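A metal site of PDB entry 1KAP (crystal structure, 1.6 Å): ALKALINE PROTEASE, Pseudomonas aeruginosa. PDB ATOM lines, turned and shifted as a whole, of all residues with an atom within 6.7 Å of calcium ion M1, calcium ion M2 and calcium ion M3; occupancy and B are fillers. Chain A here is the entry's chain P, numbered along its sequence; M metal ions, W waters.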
ATOM      1  N   GLN A 308      11.262 -38.437  -9.012  1.00  0.00           N
ATOM      2  CA  GLN A 308      10.321 -37.891  -9.984  1.00  0.00           C
ATOM      3  C   GLN A 308       9.708 -36.618  -9.431  1.00  0.00           C
ATOM      4  O   GLN A 308       9.738 -36.373  -8.217  1.00  0.00           O
ATOM      5  CB  GLN A 308       9.187 -38.891 -10.270  1.00  0.00           C
ATOM      6  CG  GLN A 308       9.610 -40.243 -10.818  1.00  0.00           C
ATOM      7  CD  GLN A 308       9.885 -41.273  -9.738  1.00  0.00           C
ATOM      8  OE1 GLN A 308       9.950 -40.950  -8.547  1.00  0.00           O
ATOM      9  NE2 GLN A 308      10.031 -42.522 -10.137  1.00  0.00           N
ATOM     10  N   GLN A 310       6.885 -34.530  -8.065  1.00  0.00           N
ATOM     11  CA  GLN A 310       5.684 -34.920  -7.360  1.00  0.00           C
ATOM     12  C   GLN A 310       4.737 -33.769  -7.074  1.00  0.00           C
ATOM     13  O   GLN A 310       5.148 -32.611  -7.095  1.00  0.00           O
ATOM     14  CB  GLN A 310       6.077 -35.622  -6.044  1.00  0.00           C
ATOM     15  CG  GLN A 310       7.077 -36.752  -6.248  1.00  0.00           C
ATOM     16  CD  GLN A 310       7.423 -37.471  -4.977  1.00  0.00           C
ATOM     17  OE1 GLN A 310       6.744 -38.424  -4.594  1.00  0.00           O
ATOM     18  NE2 GLN A 310       8.481 -37.039  -4.292  1.00  0.00           N
ATOM     19  N   GLY A 342       8.999 -33.545   0.226  1.00  0.00           N
ATOM     20  CA  GLY A 342       9.142 -33.866  -1.187  1.00  0.00           C
ATOM     21  C   GLY A 342      10.449 -34.627  -1.446  1.00  0.00           C
ATOM     22  O   GLY A 342      11.225 -34.894  -0.514  1.00  0.00           O
ATOM     23  N   GLY A 343      10.683 -34.977  -2.710  1.00  0.00           N
ATOM     24  CA  GLY A 343      11.883 -35.708  -3.077  1.00  0.00           C
ATOM     25  C   GLY A 343      12.870 -34.826  -3.814  1.00  0.00           C
ATOM     26  O   GLY A 343      12.791 -33.593  -3.765  1.00  0.00           O
ATOM     27  N   SER A 344      13.775 -35.438  -4.568  1.00  0.00           N
ATOM     28  CA  SER A 344      14.770 -34.661  -5.297  1.00  0.00           C
ATOM     29  C   SER A 344      14.288 -34.036  -6.611  1.00  0.00           C
ATOM     30  O   SER A 344      15.053 -33.347  -7.294  1.00  0.00           O
ATOM     31  CB  SER A 344      16.038 -35.487  -5.501  1.00  0.00           C
ATOM     32  OG  SER A 344      15.809 -36.598  -6.350  1.00  0.00           O
ATOM     33  N   GLY A 345      13.049 -34.284  -7.006  1.00  0.00           N
ATOM     34  CA  GLY A 345      12.530 -33.678  -8.213  1.00  0.00           C
ATOM     35  C   GLY A 345      11.938 -32.317  -7.899  1.00  0.00           C
ATOM     36  O   GLY A 345      11.983 -31.865  -6.759  1.00  0.00           O
ATOM     37  N   SER A 346      11.391 -31.646  -8.905  1.00  0.00           N
ATOM     38  CA  SER A 346      10.749 -30.349  -8.712  1.00  0.00           C
ATOM     39  C   SER A 346       9.300 -30.654  -8.318  1.00  0.00           C
ATOM     40  O   SER A 346       8.496 -31.103  -9.131  1.00  0.00           O
ATOM     41  CB  SER A 346      10.859 -29.522  -9.994  1.00  0.00           C
ATOM     42  OG  SER A 346      12.236 -29.315 -10.283  1.00  0.00           O
ATOM     43  N   ASP A 347       8.987 -30.421  -7.055  1.00  0.00           N
ATOM     44  CA  ASP A 347       7.686 -30.760  -6.483  1.00  0.00           C
ATOM     45  C   ASP A 347       6.741 -29.615  -6.214  1.00  0.00           C
ATOM     46  O   ASP A 347       7.147 -28.461  -6.117  1.00  0.00           O
ATOM     47  CB  ASP A 347       7.913 -31.492  -5.164  1.00  0.00           C
ATOM     48  CG  ASP A 347       8.911 -32.613  -5.278  1.00  0.00           C
ATOM     49  OD1 ASP A 347       8.795 -33.424  -6.219  1.00  0.00           O
ATOM     50  OD2 ASP A 347       9.817 -32.686  -4.434  1.00  0.00           O
ATOM     51  N   LEU A 349       4.024 -28.731  -3.346  1.00  0.00           N
ATOM     52  CA  LEU A 349       3.558 -29.108  -2.010  1.00  0.00           C
ATOM     53  C   LEU A 349       2.480 -28.129  -1.552  1.00  0.00           C
ATOM     54  O   LEU A 349       2.735 -26.915  -1.425  1.00  0.00           O
ATOM     55  CB  LEU A 349       4.695 -29.141  -1.001  1.00  0.00           C
ATOM     56  CG  LEU A 349       5.716 -30.265  -1.135  1.00  0.00           C
ATOM     57  CD1 LEU A 349       6.870 -29.807  -1.990  1.00  0.00           C
ATOM     58  CD2 LEU A 349       6.228 -30.627   0.231  1.00  0.00           C
ATOM     59  N   LYS A 359       8.598 -29.524   3.347  1.00  0.00           N
ATOM     60  CA  LYS A 359      10.002 -29.517   2.968  1.00  0.00           C
ATOM     61  C   LYS A 359      10.135 -29.972   1.515  1.00  0.00           C
ATOM     62  O   LYS A 359       9.767 -31.093   1.175  1.00  0.00           O
ATOM     63  CB  LYS A 359      10.812 -30.429   3.878  1.00  0.00           C
ATOM     64  CG  LYS A 359      10.747 -30.040   5.322  1.00  0.00           C
ATOM     65  CD  LYS A 359      11.724 -30.843   6.108  1.00  0.00           C
ATOM     66  CE  LYS A 359      11.730 -30.403   7.551  1.00  0.00           C
ATOM     67  NZ  LYS A 359      12.799 -31.084   8.337  1.00  0.00           N
ATOM     68  N   GLY A 360      10.656 -29.088   0.667  1.00  0.00           N
ATOM     69  CA  GLY A 360      10.784 -29.396  -0.734  1.00  0.00           C
ATOM     70  C   GLY A 360      11.932 -30.303  -1.108  1.00  0.00           C
ATOM     71  O   GLY A 360      11.820 -31.037  -2.088  1.00  0.00           O
ATOM     72  N   GLY A 361      13.010 -30.277  -0.347  1.00  0.00           N
ATOM     73  CA  GLY A 361      14.177 -31.090  -0.683  1.00  0.00           C
ATOM     74  C   GLY A 361      14.848 -30.478  -1.911  1.00  0.00           C
ATOM     75  O   GLY A 361      14.630 -29.302  -2.217  1.00  0.00           O
ATOM     76  N   ALA A 362      15.698 -31.244  -2.587  1.00  0.00           N
ATOM     77  CA  ALA A 362      16.369 -30.751  -3.791  1.00  0.00           C
ATOM     78  C   ALA A 362      15.320 -30.517  -4.884  1.00  0.00           C
ATOM     79  O   ALA A 362      14.189 -31.001  -4.779  1.00  0.00           O
ATOM     80  CB  ALA A 362      17.435 -31.754  -4.260  1.00  0.00           C
ATOM     81  N   GLY A 363      15.707 -29.823  -5.938  1.00  0.00           N
ATOM     82  CA  GLY A 363      14.789 -29.536  -7.023  1.00  0.00           C
ATOM     83  C   GLY A 363      14.150 -28.175  -6.816  1.00  0.00           C
ATOM     84  O   GLY A 363      14.203 -27.620  -5.724  1.00  0.00           O
ATOM     85  N   ASN A 364      13.568 -27.635  -7.866  1.00  0.00           N
ATOM     86  CA  ASN A 364      12.902 -26.337  -7.833  1.00  0.00           C
ATOM     87  C   ASN A 364      11.441 -26.565  -7.463  1.00  0.00           C
ATOM     88  O   ASN A 364      10.590 -26.803  -8.316  1.00  0.00           O
ATOM     89  CB  ASN A 364      13.017 -25.643  -9.196  1.00  0.00           C
ATOM     90  CG  ASN A 364      14.464 -25.281  -9.555  1.00  0.00           C
ATOM     91  OD1 ASN A 364      15.399 -25.420  -8.757  1.00  0.00           O
ATOM     92  ND2 ASN A 364      14.648 -24.810 -10.771  1.00  0.00           N
ATOM     93  N   ASP A 365      11.159 -26.469  -6.170  1.00  0.00           N
ATOM     94  CA  ASP A 365       9.840 -26.735  -5.633  1.00  0.00           C
ATOM     95  C   ASP A 365       8.947 -25.516  -5.501  1.00  0.00           C
ATOM     96  O   ASP A 365       9.432 -24.383  -5.414  1.00  0.00           O
ATOM     97  CB  ASP A 365       9.989 -27.411  -4.272  1.00  0.00           C
ATOM     98  CG  ASP A 365      10.957 -28.588  -4.315  1.00  0.00           C
ATOM     99  OD1 ASP A 365      10.651 -29.593  -4.973  1.00  0.00           O
ATOM    100  OD2 ASP A 365      12.026 -28.508  -3.687  1.00  0.00           O
ATOM    101  N   LEU A 367       5.888 -24.255  -3.034  1.00  0.00           N
ATOM    102  CA  LEU A 367       5.252 -24.547  -1.755  1.00  0.00           C
ATOM    103  C   LEU A 367       4.114 -23.577  -1.478  1.00  0.00           C
ATOM    104  O   LEU A 367       4.227 -22.377  -1.715  1.00  0.00           O
ATOM    105  CB  LEU A 367       6.302 -24.505  -0.607  1.00  0.00           C
ATOM    106  CG  LEU A 367       7.427 -25.565  -0.599  1.00  0.00           C
ATOM    107  CD1 LEU A 367       8.575 -25.112  -1.516  1.00  0.00           C
ATOM    108  CD2 LEU A 367       7.970 -25.753   0.801  1.00  0.00           C
ATOM    109  N   TRP A 377      10.309 -25.028   4.168  1.00  0.00           N
ATOM    110  CA  TRP A 377      11.698 -25.280   3.818  1.00  0.00           C
ATOM    111  C   TRP A 377      11.757 -25.572   2.326  1.00  0.00           C
ATOM    112  O   TRP A 377      11.194 -26.571   1.874  1.00  0.00           O
ATOM    113  CB  TRP A 377      12.200 -26.494   4.561  1.00  0.00           C
ATOM    114  CG  TRP A 377      12.104 -26.416   6.032  1.00  0.00           C
ATOM    115  CD1 TRP A 377      10.977 -26.604   6.825  1.00  0.00           C
ATOM    116  CD2 TRP A 377      13.183 -26.200   6.929  1.00  0.00           C
ATOM    117  NE1 TRP A 377      11.320 -26.537   8.145  1.00  0.00           N
ATOM    118  CE2 TRP A 377      12.667 -26.291   8.247  1.00  0.00           C
ATOM    119  CE3 TRP A 377      14.548 -25.963   6.746  1.00  0.00           C
ATOM    120  CZ2 TRP A 377      13.467 -26.141   9.373  1.00  0.00           C
ATOM    121  CZ3 TRP A 377      15.346 -25.808   7.863  1.00  0.00           C
ATOM    122  CH2 TRP A 377      14.808 -25.903   9.160  1.00  0.00           C
ATOM    123  N   GLY A 378      12.425 -24.722   1.551  1.00  0.00           N
ATOM    124  CA  GLY A 378      12.539 -24.980   0.135  1.00  0.00           C
ATOM    125  C   GLY A 378      13.629 -25.999  -0.194  1.00  0.00           C
ATOM    126  O   GLY A 378      13.526 -26.736  -1.178  1.00  0.00           O
ATOM    127  N   GLY A 379      14.629 -26.092   0.672  1.00  0.00           N
ATOM    128  CA  GLY A 379      15.757 -26.989   0.429  1.00  0.00           C
ATOM    129  C   GLY A 379      16.619 -26.420  -0.699  1.00  0.00           C
ATOM    130  O   GLY A 379      16.527 -25.234  -1.032  1.00  0.00           O
ATOM    131  N   ALA A 380      17.483 -27.252  -1.274  1.00  0.00           N
ATOM    132  CA  ALA A 380      18.340 -26.811  -2.380  1.00  0.00           C
ATOM    133  C   ALA A 380      17.471 -26.495  -3.580  1.00  0.00           C
ATOM    134  O   ALA A 380      16.336 -26.956  -3.677  1.00  0.00           O
ATOM    135  CB  ALA A 380      19.341 -27.909  -2.732  1.00  0.00           C
ATOM    136  N   GLY A 381      18.007 -25.716  -4.506  1.00  0.00           N
ATOM    137  CA  GLY A 381      17.264 -25.355  -5.702  1.00  0.00           C
ATOM    138  C   GLY A 381      16.531 -24.044  -5.547  1.00  0.00           C
ATOM    139  O   GLY A 381      16.487 -23.463  -4.461  1.00  0.00           O
ATOM    140  N   ALA A 382      15.967 -23.562  -6.648  1.00  0.00           N
ATOM    141  CA  ALA A 382      15.229 -22.311  -6.671  1.00  0.00           C
ATOM    142  C   ALA A 382      13.755 -22.596  -6.319  1.00  0.00           C
ATOM    143  O   ALA A 382      12.978 -23.036  -7.181  1.00  0.00           O
ATOM    144  CB  ALA A 382      15.341 -21.682  -8.048  1.00  0.00           C
ATOM    145  N   ASP A 383      13.388 -22.313  -5.083  1.00  0.00           N
ATOM    146  CA  ASP A 383      12.031 -22.579  -4.608  1.00  0.00           C
ATOM    147  C   ASP A 383      11.135 -21.358  -4.558  1.00  0.00           C
ATOM    148  O   ASP A 383      11.598 -20.242  -4.331  1.00  0.00           O
ATOM    149  CB  ASP A 383      12.123 -23.250  -3.252  1.00  0.00           C
ATOM    150  CG  ASP A 383      13.071 -24.434  -3.282  1.00  0.00           C
ATOM    151  OD1 ASP A 383      12.767 -25.427  -3.969  1.00  0.00           O
ATOM    152  OD2 ASP A 383      14.151 -24.362  -2.650  1.00  0.00           O
ATOM    153  N   PHE A 385       7.658 -19.744  -2.806  1.00  0.00           N
ATOM    154  CA  PHE A 385       6.686 -19.807  -1.718  1.00  0.00           C
ATOM    155  C   PHE A 385       5.497 -18.958  -2.168  1.00  0.00           C
ATOM    156  O   PHE A 385       5.604 -17.745  -2.324  1.00  0.00           O
ATOM    157  CB  PHE A 385       7.331 -19.308  -0.426  1.00  0.00           C
ATOM    158  CG  PHE A 385       8.591 -20.041  -0.094  1.00  0.00           C
ATOM    159  CD1 PHE A 385       8.557 -21.217   0.662  1.00  0.00           C
ATOM    160  CD2 PHE A 385       9.831 -19.600  -0.588  1.00  0.00           C
ATOM    161  CE1 PHE A 385       9.723 -21.950   0.912  1.00  0.00           C
ATOM    162  CE2 PHE A 385      10.996 -20.328  -0.347  1.00  0.00           C
ATOM    163  CZ  PHE A 385      10.946 -21.505   0.401  1.00  0.00           C
ATOM    164  N   ASP A 403      14.691 -21.405   5.307  1.00  0.00           N
ATOM    165  CA  ASP A 403      15.982 -21.512   4.640  1.00  0.00           C
ATOM    166  C   ASP A 403      16.012 -20.682   3.357  1.00  0.00           C
ATOM    167  O   ASP A 403      16.544 -21.105   2.327  1.00  0.00           O
ATOM    168  CB  ASP A 403      16.281 -22.998   4.332  1.00  0.00           C
ATOM    169  CG  ASP A 403      15.254 -23.642   3.369  1.00  0.00           C
ATOM    170  OD1 ASP A 403      14.249 -23.012   2.990  1.00  0.00           O
ATOM    171  OD2 ASP A 403      15.462 -24.805   2.979  1.00  0.00           O
ATOM    172  N   PHE A 404      15.452 -19.480   3.436  1.00  0.00           N
ATOM    173  CA  PHE A 404      15.373 -18.611   2.289  1.00  0.00           C
ATOM    174  C   PHE A 404      16.735 -18.148   1.775  1.00  0.00           C
ATOM    175  O   PHE A 404      17.569 -17.681   2.542  1.00  0.00           O
ATOM    176  CB  PHE A 404      14.504 -17.393   2.605  1.00  0.00           C
ATOM    177  CG  PHE A 404      14.029 -16.660   1.390  1.00  0.00           C
ATOM    178  CD1 PHE A 404      12.859 -17.051   0.735  1.00  0.00           C
ATOM    179  CD2 PHE A 404      14.770 -15.589   0.869  1.00  0.00           C
ATOM    180  CE1 PHE A 404      12.434 -16.395  -0.420  1.00  0.00           C
ATOM    181  CE2 PHE A 404      14.349 -14.943  -0.269  1.00  0.00           C
ATOM    182  CZ  PHE A 404      13.180 -15.334  -0.924  1.00  0.00           C
ATOM    183  N   VAL A 405      16.938 -18.273   0.474  1.00  0.00           N
ATOM    184  CA  VAL A 405      18.195 -17.855  -0.146  1.00  0.00           C
ATOM    185  C   VAL A 405      17.901 -16.814  -1.227  1.00  0.00           C
ATOM    186  O   VAL A 405      17.315 -17.131  -2.272  1.00  0.00           O
ATOM    187  CB  VAL A 405      18.944 -19.051  -0.775  1.00  0.00           C
ATOM    188  CG1 VAL A 405      20.200 -18.580  -1.482  1.00  0.00           C
ATOM    189  CG2 VAL A 405      19.288 -20.064   0.298  1.00  0.00           C
ATOM    190  N   GLN A 408      17.833 -16.861  -5.312  1.00  0.00           N
ATOM    191  CA  GLN A 408      17.490 -18.228  -5.720  1.00  0.00           C
ATOM    192  C   GLN A 408      16.002 -18.467  -5.480  1.00  0.00           C
ATOM    193  O   GLN A 408      15.266 -18.758  -6.421  1.00  0.00           O
ATOM    194  CB  GLN A 408      18.300 -19.265  -4.956  1.00  0.00           C
ATOM    195  CG  GLN A 408      19.413 -19.895  -5.790  1.00  0.00           C
ATOM    196  CD  GLN A 408      19.664 -21.350  -5.409  1.00  0.00           C
ATOM    197  OE1 GLN A 408      19.868 -21.667  -4.231  1.00  0.00           O
ATOM    198  NE2 GLN A 408      19.652 -22.237  -6.399  1.00  0.00           N
ATOM    199  N   ASP A 409      15.574 -18.324  -4.239  1.00  0.00           N
ATOM    200  CA  ASP A 409      14.163 -18.525  -3.902  1.00  0.00           C
ATOM    201  C   ASP A 409      13.344 -17.270  -4.188  1.00  0.00           C
ATOM    202  O   ASP A 409      13.903 -16.186  -4.388  1.00  0.00           O
ATOM    203  CB  ASP A 409      14.014 -18.914  -2.432  1.00  0.00           C
ATOM    204  CG  ASP A 409      14.825 -20.131  -2.062  1.00  0.00           C
ATOM    205  OD1 ASP A 409      14.946 -21.071  -2.869  1.00  0.00           O
ATOM    206  OD2 ASP A 409      15.336 -20.149  -0.945  1.00  0.00           O
HETATM  207 CA    CA M   1      11.940 -31.493  -4.387  1.00  0.00          CA
HETATM  208 CA    CA M   2      14.034 -27.348  -3.341  1.00  0.00          CA
HETATM  209 CA    CA M   3      15.984 -23.170  -2.082  1.00  0.00          CA
HETATM  210  O   HOH W   1      18.259 -22.627  -1.961  1.00  0.00           O
HETATM  211  O   HOH W   2      15.013 -22.564   0.060  1.00  0.00           O
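Water W2 lies within hydrogen-bond range of OD2 of Asp 409 and OD1 of Asp 403.
Seven residues have an atom within 4 Å of calcium ion M1: Gly 343, Gly 345, Asp 347, Gly 360, Gly 361, Ala 362 and Asp 365.
Calcium ion M3 is bound by OD2 of Asp 383 (2.3 Å), water W1 (2.3 Å), O of Gly 379 (2.4 Å), water W2 (2.4 Å), O of Gly 381 (2.4 Å) and OD1 of Asp 409 (2.5 Å).
Calcium ion M3 has six donor atoms within binding distance.
Calcium ion M1 is bound by the backbone carbonyl oxygen of Ala 362, the backbone carbonyl oxygen of Gly 360, the backbone carbonyl oxygen of Gly 343, the side-chain carboxylate of Asp 365, the backbone carbonyl oxygen of Gly 345 and the side-chain carboxylate of Asp 347.
Calcium ion M1 has six donor atoms within binding distance.
Slightly farther from calcium ion M1 lies the side-chain carboxylate (OD2) of Asp 365 (3.1 Å).
Calcium ion M2 is bound by O of Gly 378 (2.3 Å), O of Gly 361 (2.3 Å), OD2 of Asp 365 (2.3 Å), O of Ala 380 (2.4 Å), OD1 of Asp 383 (2.4 Å) and O of Gly 363 (2.4 Å).
Calcium ion M2 has six donor atoms within binding distance.
Slightly farther from calcium ion M2 lies OD2 of Asp 383 (3.1 Å).
Eight residues have an atom within 4 Å of calcium ion M2: Gly 361, Ala 362, Gly 363, Asp 365, Gly 378, Gly 379, Ala 380 and Asp 383.
The backbone NH (N) of Gly 378 sits at hydrogen-bond distance from the side-chain carboxylate (OD1) of Asp 403 (2.9 Å).
The backbone NH (N) of Gly 379 lies within hydrogen-bond range of the side-chain carboxylate (OD2) of Asp 403 (2.8 Å).
NE2 of Gln 310 sits close to N of Gly 343.
OD1 of Asp 347 is in hydrogen-bond range of N of Gln 310.
The backbone NH (N) of Gly 360 is in hydrogen-bond range of the backbone carbonyl oxygen (O) of Trp 377, 2.8 Å away.
The backbone NH of Val 405 is in hydrogen-bond range of the side-chain carboxylate of Asp 409 (2.8 Å).
Five residues have an atom within 4 Å of calcium ion M3: Gly 379, Ala 380, Gly 381, Asp 383 and Asp 409.
The nearest printed residue that does not touch calcium ion M3 is Gly 378 (4.1 Å).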
